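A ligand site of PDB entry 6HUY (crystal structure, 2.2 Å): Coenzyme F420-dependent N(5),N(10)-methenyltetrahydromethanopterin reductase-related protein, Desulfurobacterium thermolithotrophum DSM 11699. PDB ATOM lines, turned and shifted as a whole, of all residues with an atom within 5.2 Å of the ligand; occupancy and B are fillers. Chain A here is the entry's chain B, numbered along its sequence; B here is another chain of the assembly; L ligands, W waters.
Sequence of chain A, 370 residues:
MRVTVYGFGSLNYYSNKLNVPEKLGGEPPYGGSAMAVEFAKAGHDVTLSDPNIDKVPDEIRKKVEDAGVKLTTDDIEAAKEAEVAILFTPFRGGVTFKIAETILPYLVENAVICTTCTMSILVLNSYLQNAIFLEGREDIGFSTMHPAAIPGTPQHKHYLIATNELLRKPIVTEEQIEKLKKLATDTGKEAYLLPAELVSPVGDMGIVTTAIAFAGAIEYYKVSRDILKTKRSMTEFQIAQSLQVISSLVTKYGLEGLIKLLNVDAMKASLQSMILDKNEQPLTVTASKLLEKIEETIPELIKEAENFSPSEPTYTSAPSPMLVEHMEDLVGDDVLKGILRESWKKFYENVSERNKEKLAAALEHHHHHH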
ATOM      1  N   SER A  10       7.753  -7.671  10.931  1.00  0.00           N
ATOM      2  CA  SER A  10       9.160  -8.012  11.123  1.00  0.00           C
ATOM      3  C   SER A  10      10.024  -7.414  10.029  1.00  0.00           C
ATOM      4  O   SER A  10      10.012  -7.891   8.897  1.00  0.00           O
ATOM      5  CB  SER A  10       9.365  -9.526  11.153  1.00  0.00           C
ATOM      6  OG  SER A  10      10.747  -9.829  11.217  1.00  0.00           O
ATOM      7  N   TYR A  13      12.129 -10.048   8.519  1.00  0.00           N
ATOM      8  CA  TYR A  13      11.464 -10.991   7.624  1.00  0.00           C
ATOM      9  C   TYR A  13      11.319 -10.375   6.238  1.00  0.00           C
ATOM     10  O   TYR A  13      11.693 -10.986   5.228  1.00  0.00           O
ATOM     11  CB  TYR A  13      10.092 -11.416   8.160  1.00  0.00           C
ATOM     12  CG  TYR A  13       9.374 -12.264   7.145  1.00  0.00           C
ATOM     13  CD1 TYR A  13       9.675 -13.609   7.007  1.00  0.00           C
ATOM     14  CD2 TYR A  13       8.458 -11.704   6.264  1.00  0.00           C
ATOM     15  CE1 TYR A  13       9.072 -14.378   6.039  1.00  0.00           C
ATOM     16  CE2 TYR A  13       7.837 -12.461   5.288  1.00  0.00           C
ATOM     17  CZ  TYR A  13       8.156 -13.798   5.189  1.00  0.00           C
ATOM     18  OH  TYR A  13       7.553 -14.566   4.222  1.00  0.00           O
ATOM     19  N   TYR A  14      10.795  -9.153   6.177  1.00  0.00           N
ATOM     20  CA  TYR A  14      10.512  -8.474   4.921  1.00  0.00           C
ATOM     21  C   TYR A  14      11.749  -8.022   4.161  1.00  0.00           C
ATOM     22  O   TYR A  14      11.590  -7.457   3.069  1.00  0.00           O
ATOM     23  CB  TYR A  14       9.639  -7.250   5.200  1.00  0.00           C
ATOM     24  CG  TYR A  14       8.230  -7.571   5.634  1.00  0.00           C
ATOM     25  CD1 TYR A  14       7.445  -8.465   4.930  1.00  0.00           C
ATOM     26  CD2 TYR A  14       7.670  -6.946   6.747  1.00  0.00           C
ATOM     27  CE1 TYR A  14       6.150  -8.746   5.318  1.00  0.00           C
ATOM     28  CE2 TYR A  14       6.392  -7.215   7.142  1.00  0.00           C
ATOM     29  CZ  TYR A  14       5.636  -8.117   6.428  1.00  0.00           C
ATOM     30  OH  TYR A  14       4.350  -8.378   6.815  1.00  0.00           O
ATOM     31  N   LEU A  18      12.281 -12.775   2.916  1.00  0.00           N
ATOM     32  CA  LEU A  18      11.544 -12.500   1.696  1.00  0.00           C
ATOM     33  C   LEU A  18      11.924 -11.092   1.256  1.00  0.00           C
ATOM     34  O   LEU A  18      11.593 -10.114   1.935  1.00  0.00           O
ATOM     35  CB  LEU A  18      10.036 -12.598   1.939  1.00  0.00           C
ATOM     36  CG  LEU A  18       9.114 -12.279   0.759  1.00  0.00           C
ATOM     37  CD1 LEU A  18       9.166 -13.389  -0.273  1.00  0.00           C
ATOM     38  CD2 LEU A  18       7.692 -12.044   1.229  1.00  0.00           C
ATOM     39  N   LEU A  24       8.164  -7.701  -4.722  1.00  0.00           N
ATOM     40  CA  LEU A  24       6.890  -7.001  -4.812  1.00  0.00           C
ATOM     41  C   LEU A  24       7.039  -5.503  -5.035  1.00  0.00           C
ATOM     42  O   LEU A  24       6.362  -4.947  -5.921  1.00  0.00           O
ATOM     43  CB  LEU A  24       6.062  -7.272  -3.553  1.00  0.00           C
ATOM     44  CG  LEU A  24       5.567  -8.717  -3.449  1.00  0.00           C
ATOM     45  CD1 LEU A  24       5.210  -9.040  -2.024  1.00  0.00           C
ATOM     46  CD2 LEU A  24       4.381  -8.931  -4.363  1.00  0.00           C
ATOM     47  N   THR A  89      -0.748  -9.626  14.183  1.00  0.00           N
ATOM     48  CA  THR A  89      -0.082 -10.424  15.206  1.00  0.00           C
ATOM     49  C   THR A  89       0.244 -11.832  14.694  1.00  0.00           C
ATOM     50  O   THR A  89      -0.322 -12.291  13.699  1.00  0.00           O
ATOM     51  CB  THR A  89      -0.969 -10.528  16.451  1.00  0.00           C
ATOM     52  OG1 THR A  89      -2.329 -10.841  16.064  1.00  0.00           O
ATOM     53  CG2 THR A  89      -0.963  -9.196  17.190  1.00  0.00           C
ATOM     54  N   PRO A  90       1.132 -12.547  15.375  1.00  0.00           N
ATOM     55  CA  PRO A  90       1.524 -13.885  14.880  1.00  0.00           C
ATOM     56  C   PRO A  90       0.406 -14.928  14.968  1.00  0.00           C
ATOM     57  O   PRO A  90      -0.389 -14.982  15.918  1.00  0.00           O
ATOM     58  CB  PRO A  90       2.718 -14.264  15.763  1.00  0.00           C
ATOM     59  CG  PRO A  90       3.203 -12.965  16.349  1.00  0.00           C
ATOM     60  CD  PRO A  90       1.979 -12.117  16.503  1.00  0.00           C
ATOM     61  N   PHE A  91       0.358 -15.770  13.929  1.00  0.00           N
ATOM     62  CA  PHE A  91      -0.439 -16.990  13.916  1.00  0.00           C
ATOM     63  C   PHE A  91       0.057 -17.976  14.969  1.00  0.00           C
ATOM     64  O   PHE A  91      -0.748 -18.670  15.604  1.00  0.00           O
ATOM     65  CB  PHE A  91      -0.349 -17.616  12.515  1.00  0.00           C
ATOM     66  CG  PHE A  91      -0.855 -19.033  12.422  1.00  0.00           C
ATOM     67  CD1 PHE A  91       0.006 -20.104  12.589  1.00  0.00           C
ATOM     68  CD2 PHE A  91      -2.190 -19.278  12.121  1.00  0.00           C
ATOM     69  CE1 PHE A  91      -0.463 -21.411  12.481  1.00  0.00           C
ATOM     70  CE2 PHE A  91      -2.663 -20.568  12.009  1.00  0.00           C
ATOM     71  CZ  PHE A  91      -1.799 -21.635  12.189  1.00  0.00           C
ATOM     72  N   ARG A  92       1.370 -18.057  15.141  1.00  0.00           N
ATOM     73  CA  ARG A  92       1.965 -19.105  15.951  1.00  0.00           C
ATOM     74  C   ARG A  92       1.717 -18.870  17.440  1.00  0.00           C
ATOM     75  O   ARG A  92       1.459 -17.746  17.894  1.00  0.00           O
ATOM     76  CB  ARG A  92       3.460 -19.176  15.646  1.00  0.00           C
ATOM     77  CG  ARG A  92       4.298 -18.482  16.687  1.00  0.00           C
ATOM     78  CD  ARG A  92       5.599 -17.898  16.165  1.00  0.00           C
ATOM     79  NE  ARG A  92       5.786 -16.553  16.724  1.00  0.00           N
ATOM     80  CZ  ARG A  92       5.756 -16.244  18.020  1.00  0.00           C
ATOM     81  NH1 ARG A  92       5.554 -17.178  18.955  1.00  0.00           N
ATOM     82  NH2 ARG A  92       5.925 -14.985  18.398  1.00  0.00           N
ATOM     83  N   CSO A 117      -3.864 -11.021   8.074  1.00  0.00           N
ATOM     84  CA  CSO A 117      -3.527 -12.212   7.252  1.00  0.00           C
ATOM     85  CB  CSO A 117      -2.383 -11.912   6.274  1.00  0.00           C
ATOM     86  SG  CSO A 117      -0.893 -11.341   7.048  1.00  0.00           S
ATOM     87  C   CSO A 117      -3.141 -13.450   8.011  1.00  0.00           C
ATOM     88  O   CSO A 117      -2.908 -14.481   7.363  1.00  0.00           O
ATOM     89  OD  CSO A 117      -1.054  -9.624   6.978  1.00  0.00           O
ATOM     90  N   THR A 118      -3.068 -13.382   9.327  1.00  0.00           N
ATOM     91  CA  THR A 118      -2.523 -14.488  10.106  1.00  0.00           C
ATOM     92  C   THR A 118      -3.583 -15.348  10.836  1.00  0.00           C
ATOM     93  O   THR A 118      -3.255 -16.395  11.406  1.00  0.00           O
ATOM     94  CB  THR A 118      -1.542 -13.969  11.167  1.00  0.00           C
ATOM     95  OG1 THR A 118      -2.114 -12.837  11.816  1.00  0.00           O
ATOM     96  CG2 THR A 118      -0.234 -13.571  10.524  1.00  0.00           C
ATOM     97  N   HIS A 146      -8.082  -7.226   6.253  1.00  0.00           N
ATOM     98  CA  HIS A 146      -7.143  -8.124   5.607  1.00  0.00           C
ATOM     99  C   HIS A 146      -6.571  -7.424   4.389  1.00  0.00           C
ATOM    100  O   HIS A 146      -7.293  -7.180   3.420  1.00  0.00           O
ATOM    101  CB  HIS A 146      -7.831  -9.435   5.198  1.00  0.00           C
ATOM    102  CG  HIS A 146      -6.878 -10.553   4.919  1.00  0.00           C
ATOM    103  ND1 HIS A 146      -5.652 -10.350   4.336  1.00  0.00           N
ATOM    104  CD2 HIS A 146      -6.972 -11.883   5.164  1.00  0.00           C
ATOM    105  CE1 HIS A 146      -5.022 -11.506   4.231  1.00  0.00           C
ATOM    106  NE2 HIS A 146      -5.798 -12.457   4.716  1.00  0.00           N
ATOM    107  N   ALA A 148      -4.779  -8.551   2.068  1.00  0.00           N
ATOM    108  CA  ALA A 148      -4.702  -9.412   0.894  1.00  0.00           C
ATOM    109  C   ALA A 148      -3.510  -8.999   0.035  1.00  0.00           C
ATOM    110  O   ALA A 148      -3.566  -9.017  -1.203  1.00  0.00           O
ATOM    111  CB  ALA A 148      -5.999  -9.374   0.095  1.00  0.00           C
ATOM    112  N   ALA A 149      -2.422  -8.652   0.720  1.00  0.00           N
ATOM    113  CA  ALA A 149      -1.212  -8.068   0.165  1.00  0.00           C
ATOM    114  C   ALA A 149      -0.330  -7.665   1.340  1.00  0.00           C
ATOM    115  O   ALA A 149      -0.789  -7.656   2.478  1.00  0.00           O
ATOM    116  CB  ALA A 149      -1.505  -6.849  -0.722  1.00  0.00           C
ATOM    117  N   ILE A 150       0.914  -7.320   1.070  1.00  0.00           N
ATOM    118  CA  ILE A 150       1.788  -6.737   2.080  1.00  0.00           C
ATOM    119  C   ILE A 150       1.537  -5.235   2.094  1.00  0.00           C
ATOM    120  O   ILE A 150       1.814  -4.564   1.079  1.00  0.00           O
ATOM    121  CB  ILE A 150       3.273  -7.032   1.799  1.00  0.00           C
ATOM    122  CG1 ILE A 150       3.504  -8.544   1.724  1.00  0.00           C
ATOM    123  CG2 ILE A 150       4.127  -6.407   2.890  1.00  0.00           C
ATOM    124  CD1 ILE A 150       4.970  -8.961   1.488  1.00  0.00           C
ATOM    125  N   GLY A 203      -7.970 -14.014   1.070  1.00  0.00           N
ATOM    126  CA  GLY A 203      -6.925 -13.040   1.348  1.00  0.00           C
ATOM    127  C   GLY A 203      -5.564 -13.585   1.733  1.00  0.00           C
ATOM    128  O   GLY A 203      -4.551 -12.925   1.492  1.00  0.00           O
ATOM    129  N   ASP A 204      -5.518 -14.775   2.329  1.00  0.00           N
ATOM    130  CA  ASP A 204      -4.288 -15.342   2.863  1.00  0.00           C
ATOM    131  C   ASP A 204      -3.336 -15.724   1.737  1.00  0.00           C
ATOM    132  O   ASP A 204      -3.693 -15.737   0.562  1.00  0.00           O
ATOM    133  CB  ASP A 204      -4.585 -16.576   3.714  1.00  0.00           C
ATOM    134  CG  ASP A 204      -5.251 -16.249   5.049  1.00  0.00           C
ATOM    135  OD1 ASP A 204      -5.368 -15.064   5.415  1.00  0.00           O
ATOM    136  OD2 ASP A 204      -5.660 -17.218   5.736  1.00  0.00           O
ATOM    137  N   MET A 205      -2.097 -16.074   2.113  1.00  0.00           N
ATOM    138  CA  MET A 205      -1.150 -16.669   1.180  1.00  0.00           C
ATOM    139  C   MET A 205      -1.741 -17.889   0.461  1.00  0.00           C
ATOM    140  O   MET A 205      -1.417 -18.148  -0.702  1.00  0.00           O
ATOM    141  CB  MET A 205       0.135 -17.067   1.913  1.00  0.00           C
ATOM    142  CG  MET A 205       0.899 -15.878   2.477  1.00  0.00           C
ATOM    143  SD  MET A 205       2.256 -16.296   3.604  1.00  0.00           S
ATOM    144  CE  MET A 205       1.327 -16.845   5.038  1.00  0.00           C
ATOM    145  N   ILE A 207      -4.325 -18.158  -0.987  1.00  0.00           N
ATOM    146  CA  ILE A 207      -5.061 -17.834  -2.208  1.00  0.00           C
ATOM    147  C   ILE A 207      -4.518 -18.660  -3.365  1.00  0.00           C
ATOM    148  O   ILE A 207      -5.241 -18.935  -4.335  1.00  0.00           O
ATOM    149  CB  ILE A 207      -4.954 -16.322  -2.495  1.00  0.00           C
ATOM    150  CG1 ILE A 207      -5.793 -15.930  -3.733  1.00  0.00           C
ATOM    151  CG2 ILE A 207      -3.495 -15.917  -2.724  1.00  0.00           C
ATOM    152  CD1 ILE A 207      -7.301 -16.273  -3.659  1.00  0.00           C
ATOM    153  N   LEU B 228       8.484 -18.030   0.632  1.00  0.00           N
ATOM    154  CA  LEU B 228       7.930 -17.354   1.811  1.00  0.00           C
ATOM    155  C   LEU B 228       8.630 -17.745   3.108  1.00  0.00           C
ATOM    156  O   LEU B 228       8.612 -16.967   4.069  1.00  0.00           O
ATOM    157  CB  LEU B 228       6.448 -17.675   1.963  1.00  0.00           C
ATOM    158  CG  LEU B 228       5.490 -17.248   0.845  1.00  0.00           C
ATOM    159  CD1 LEU B 228       4.180 -17.916   1.123  1.00  0.00           C
ATOM    160  CD2 LEU B 228       5.338 -15.735   0.789  1.00  0.00           C
ATOM    161  N   THR B 230       7.782 -19.813   5.408  1.00  0.00           N
ATOM    162  CA  THR B 230       6.783 -19.898   6.473  1.00  0.00           C
ATOM    163  C   THR B 230       6.657 -21.318   7.015  1.00  0.00           C
ATOM    164  O   THR B 230       7.144 -22.278   6.418  1.00  0.00           O
ATOM    165  CB  THR B 230       5.433 -19.408   5.967  1.00  0.00           C
ATOM    166  OG1 THR B 230       5.168 -20.011   4.696  1.00  0.00           O
ATOM    167  CG2 THR B 230       5.417 -17.897   5.829  1.00  0.00           C
ATOM    168  N   MET B 234       1.089 -23.206   9.378  1.00  0.00           N
ATOM    169  CA  MET B 234       0.337 -22.118   8.740  1.00  0.00           C
ATOM    170  C   MET B 234      -0.072 -22.508   7.323  1.00  0.00           C
ATOM    171  O   MET B 234      -1.214 -22.278   6.898  1.00  0.00           O
ATOM    172  CB  MET B 234       1.197 -20.856   8.757  1.00  0.00           C
ATOM    173  CG  MET B 234       0.534 -19.581   8.220  1.00  0.00           C
ATOM    174  SD  MET B 234       1.207 -18.058   8.957  1.00  0.00           S
ATOM    175  CE  MET B 234       2.908 -18.238   8.523  1.00  0.00           C
ATOM    176  N   SER B 270      -6.029 -10.265  -4.700  1.00  0.00           N
ATOM    177  CA  SER B 270      -5.228 -10.953  -3.690  1.00  0.00           C
ATOM    178  C   SER B 270      -4.100 -11.748  -4.336  1.00  0.00           C
ATOM    179  O   SER B 270      -2.954 -11.704  -3.881  1.00  0.00           O
ATOM    180  CB  SER B 270      -6.120 -11.871  -2.855  1.00  0.00           C
ATOM    181  OG  SER B 270      -5.336 -12.676  -1.985  1.00  0.00           O
ATOM    182  N   LEU B 271      -4.412 -12.489  -5.397  1.00  0.00           N
ATOM    183  CA  LEU B 271      -3.450 -13.390  -6.010  1.00  0.00           C
ATOM    184  C   LEU B 271      -2.242 -12.664  -6.581  1.00  0.00           C
ATOM    185  O   LEU B 271      -1.181 -13.285  -6.746  1.00  0.00           O
ATOM    186  CB  LEU B 271      -4.161 -14.183  -7.121  1.00  0.00           C
ATOM    187  CG  LEU B 271      -3.485 -15.411  -7.699  1.00  0.00           C
ATOM    188  CD1 LEU B 271      -3.184 -16.442  -6.634  1.00  0.00           C
ATOM    189  CD2 LEU B 271      -4.405 -15.988  -8.777  1.00  0.00           C
ATOM    190  N   SER B 273      -0.240 -10.663  -5.194  1.00  0.00           N
ATOM    191  CA  SER B 273       0.842 -10.616  -4.232  1.00  0.00           C
ATOM    192  C   SER B 273       1.392 -11.990  -3.905  1.00  0.00           C
ATOM    193  O   SER B 273       2.269 -12.114  -3.062  1.00  0.00           O
ATOM    194  CB  SER B 273       0.367  -9.926  -2.961  1.00  0.00           C
ATOM    195  OG  SER B 273       0.251  -8.527  -3.193  1.00  0.00           O
ATOM    196  N   MET B 274       0.892 -13.037  -4.572  1.00  0.00           N
ATOM    197  CA  MET B 274       1.370 -14.386  -4.352  1.00  0.00           C
ATOM    198  C   MET B 274       1.960 -15.018  -5.606  1.00  0.00           C
ATOM    199  O   MET B 274       2.251 -16.213  -5.595  1.00  0.00           O
ATOM    200  CB  MET B 274       0.251 -15.255  -3.797  1.00  0.00           C
ATOM    201  CG  MET B 274       0.083 -15.114  -2.294  1.00  0.00           C
ATOM    202  SD  MET B 274       1.624 -15.454  -1.407  1.00  0.00           S
ATOM    203  CE  MET B 274       1.855 -17.187  -1.827  1.00  0.00           C
ATOM    204  N   LEU B 276       5.028 -15.075  -6.947  1.00  0.00           N
ATOM    205  CA  LEU B 276       6.378 -14.710  -6.561  1.00  0.00           C
ATOM    206  C   LEU B 276       7.460 -15.387  -7.380  1.00  0.00           C
ATOM    207  O   LEU B 276       8.619 -14.957  -7.340  1.00  0.00           O
ATOM    208  CB  LEU B 276       6.604 -15.037  -5.076  1.00  0.00           C
ATOM    209  CG  LEU B 276       5.605 -14.365  -4.128  1.00  0.00           C
ATOM    210  CD1 LEU B 276       5.557 -15.109  -2.809  1.00  0.00           C
ATOM    211  CD2 LEU B 276       5.996 -12.904  -3.910  1.00  0.00           C
HETATM  212  N1  LIG L   1      -0.236 -12.212  -0.451  1.00  0.00           N
HETATM  213  C1  LIG L   1      -1.499 -12.336   0.030  1.00  0.00           C
HETATM  214  N2  LIG L   1      -1.762 -12.502   1.337  1.00  0.00           N
HETATM  215  C2  LIG L   1      -0.782 -12.554   2.255  1.00  0.00           C
HETATM  216  C3  LIG L   1       3.060 -12.057   2.107  1.00  0.00           C
HETATM  217  C4  LIG L   1       4.226 -14.695   7.888  1.00  0.00           C
HETATM  218  C5  LIG L   1       2.952 -14.136   7.738  1.00  0.00           C
HETATM  219  C6  LIG L   1       2.560 -13.558   6.525  1.00  0.00           C
HETATM  220  C7  LIG L   1       3.434 -13.507   5.452  1.00  0.00           C
HETATM  221  C8  LIG L   1       4.701 -14.079   5.585  1.00  0.00           C
HETATM  222  O1  LIG L   1      -1.075 -12.698   3.447  1.00  0.00           O
HETATM  223  C9  LIG L   1       0.629 -12.424   1.817  1.00  0.00           C
HETATM  224  N3  LIG L   1       1.772 -12.445   2.659  1.00  0.00           N
HETATM  225  C10 LIG L   1       3.145 -12.723   0.722  1.00  0.00           C
HETATM  226  N4  LIG L   1       2.101 -12.138  -0.110  1.00  0.00           N
HETATM  227  C11 LIG L   1       0.846 -12.242   0.369  1.00  0.00           C
HETATM  228  N5  LIG L   1      -2.527 -12.296  -0.866  1.00  0.00           N
HETATM  229  C12 LIG L   1       4.010 -12.641   3.157  1.00  0.00           C
HETATM  230  N6  LIG L   1       3.054 -12.946   4.211  1.00  0.00           N
HETATM  231  C13 LIG L   1       5.098 -14.669   6.793  1.00  0.00           C
HETATM  232  C14 LIG L   1       4.644 -15.349   9.182  1.00  0.00           C
HETATM  233  O2  LIG L   1       5.426 -16.298   9.150  1.00  0.00           O
HETATM  234  N7  LIG L   1       4.134 -14.967  10.351  1.00  0.00           N
HETATM  235  C15 LIG L   1       4.399 -15.755  11.548  1.00  0.00           C
HETATM  236  C16 LIG L   1       3.137 -16.179  12.251  1.00  0.00           C
HETATM  237  O3  LIG L   1       3.136 -17.259  12.887  1.00  0.00           O
HETATM  238  O4  LIG L   1       2.143 -15.421  12.187  1.00  0.00           O
HETATM  239  C17 LIG L   1       5.205 -14.927  12.543  1.00  0.00           C
HETATM  240  C18 LIG L   1       6.694 -15.260  12.586  1.00  0.00           C
HETATM  241  C19 LIG L   1       7.243 -14.498  13.773  1.00  0.00           C
HETATM  242  O5  LIG L   1       7.661 -13.316  13.614  1.00  0.00           O
HETATM  243  O6  LIG L   1       7.236 -15.072  14.895  1.00  0.00           O
HETATM  244  C20 LIG L   1       1.842 -12.762   3.877  1.00  0.00           C
HETATM  245  O   HOH W   1       4.371 -19.326  12.143  1.00  0.00           O
HETATM  246  O   HOH W   2       2.652  -9.808   5.521  1.00  0.00           O
HETATM  247  O   HOH W   3      -1.596 -15.234   4.715  1.00  0.00           O
HETATM  248  O   HOH W   4       5.384 -18.771   9.760  1.00  0.00           O
HETATM  249  O   HOH W   5       2.806 -11.946  10.711  1.00  0.00           O
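Water W3 lies within hydrogen-bond range of the backbone NH of Met 205, an oxygen (O1) of the ligand and O of CSO 117.
The side-chain sulfur of Met 205 sits close to a nitrogen (N6) of the ligand. Merely in contact with the ligand: Pro 90 (3.2 Å), Tyr 13 (3.2 Å), CSO 117 (3.2 Å), Met 234 of chain B (3.2 Å), Thr 230 of chain B (3.4 Å), Thr 118 (3.4 Å), Ile 150 (3.6 Å), Asp 204 (3.6 Å), Leu 228 of chain B (3.7 Å) and Ala 149 (3.9 Å). Hydrophobic or aromatic side chains that line the ligand: Tyr 13, Pro 90, Phe 91, Ile 150, Met 205, Leu 228 of chain B, Met 234 of chain B and Met 274 of chain B. Of the 27 residues printed, 18 come within 4 Å of the ligand. Along chain A the residues within 4 Å of the ligand span positions 13 to 205. The nearest printed residue that does not touch the ligand is Ile 207 (4.2 Å).
The backbone NH (N) of Phe 91 lies within hydrogen-bond range of an oxygen (O4) of the ligand, 2.5 Å away. O3 of the ligand lies within hydrogen-bond range of N of Arg 92 (3.0 Å). An oxygen (O6) of the ligand is in salt-bridge range of the guanidinium group (NE) of Arg 92, 2.8 Å away. O of Gly 203 sits at hydrogen-bond distance from N5 of the ligand, at 3.2 Å. O of Ser 273 of chain B lies within hydrogen-bond range of N4 of the ligand (3.0 Å). The backbone carbonyl oxygen (O) of Ser 270 of chain B is in hydrogen-bond range of a nitrogen (N5) of the ligand (3.1 Å). A nitrogen (N5) of the ligand sits at hydrogen-bond distance from the side-chain hydroxyl (OG) of Ser 270 of chain B (3.0 Å). A nitrogen (N4) of the ligand lies within hydrogen-bond range of the side-chain sulfur (SD) of Met 274 of chain B. The backbone carbonyl oxygen (O) of Ala 148 is in hydrogen-bond range of a nitrogen (N5) of the ligand (3.5 Å).
NE2 of His 146 sits close to O of Gly 203 (3.5 Å). OH of Tyr 13 sits at hydrogen-bond distance from O of Leu 228 of chain B, at 2.6 Å. N of Leu 18 is in hydrogen-bond range of O of Tyr 13, at 3.0 Å. The backbone NH (N) of Tyr 13 is in hydrogen-bond range of the side-chain hydroxyl (OG) of Ser 10, at 3.0 Å. The backbone carbonyl oxygen (O) of Thr 89 sits at hydrogen-bond distance from the side-chain hydroxyl (OG1) of Thr 118. A ring nitrogen (ND1) of His 146 lies within hydrogen-bond range of the backbone NH (N) of Ala 148 (3.0 Å). The side-chain carboxylate (OD1) of Asp 204 lies within hydrogen-bond range of a ring nitrogen (NE2) of His 146.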
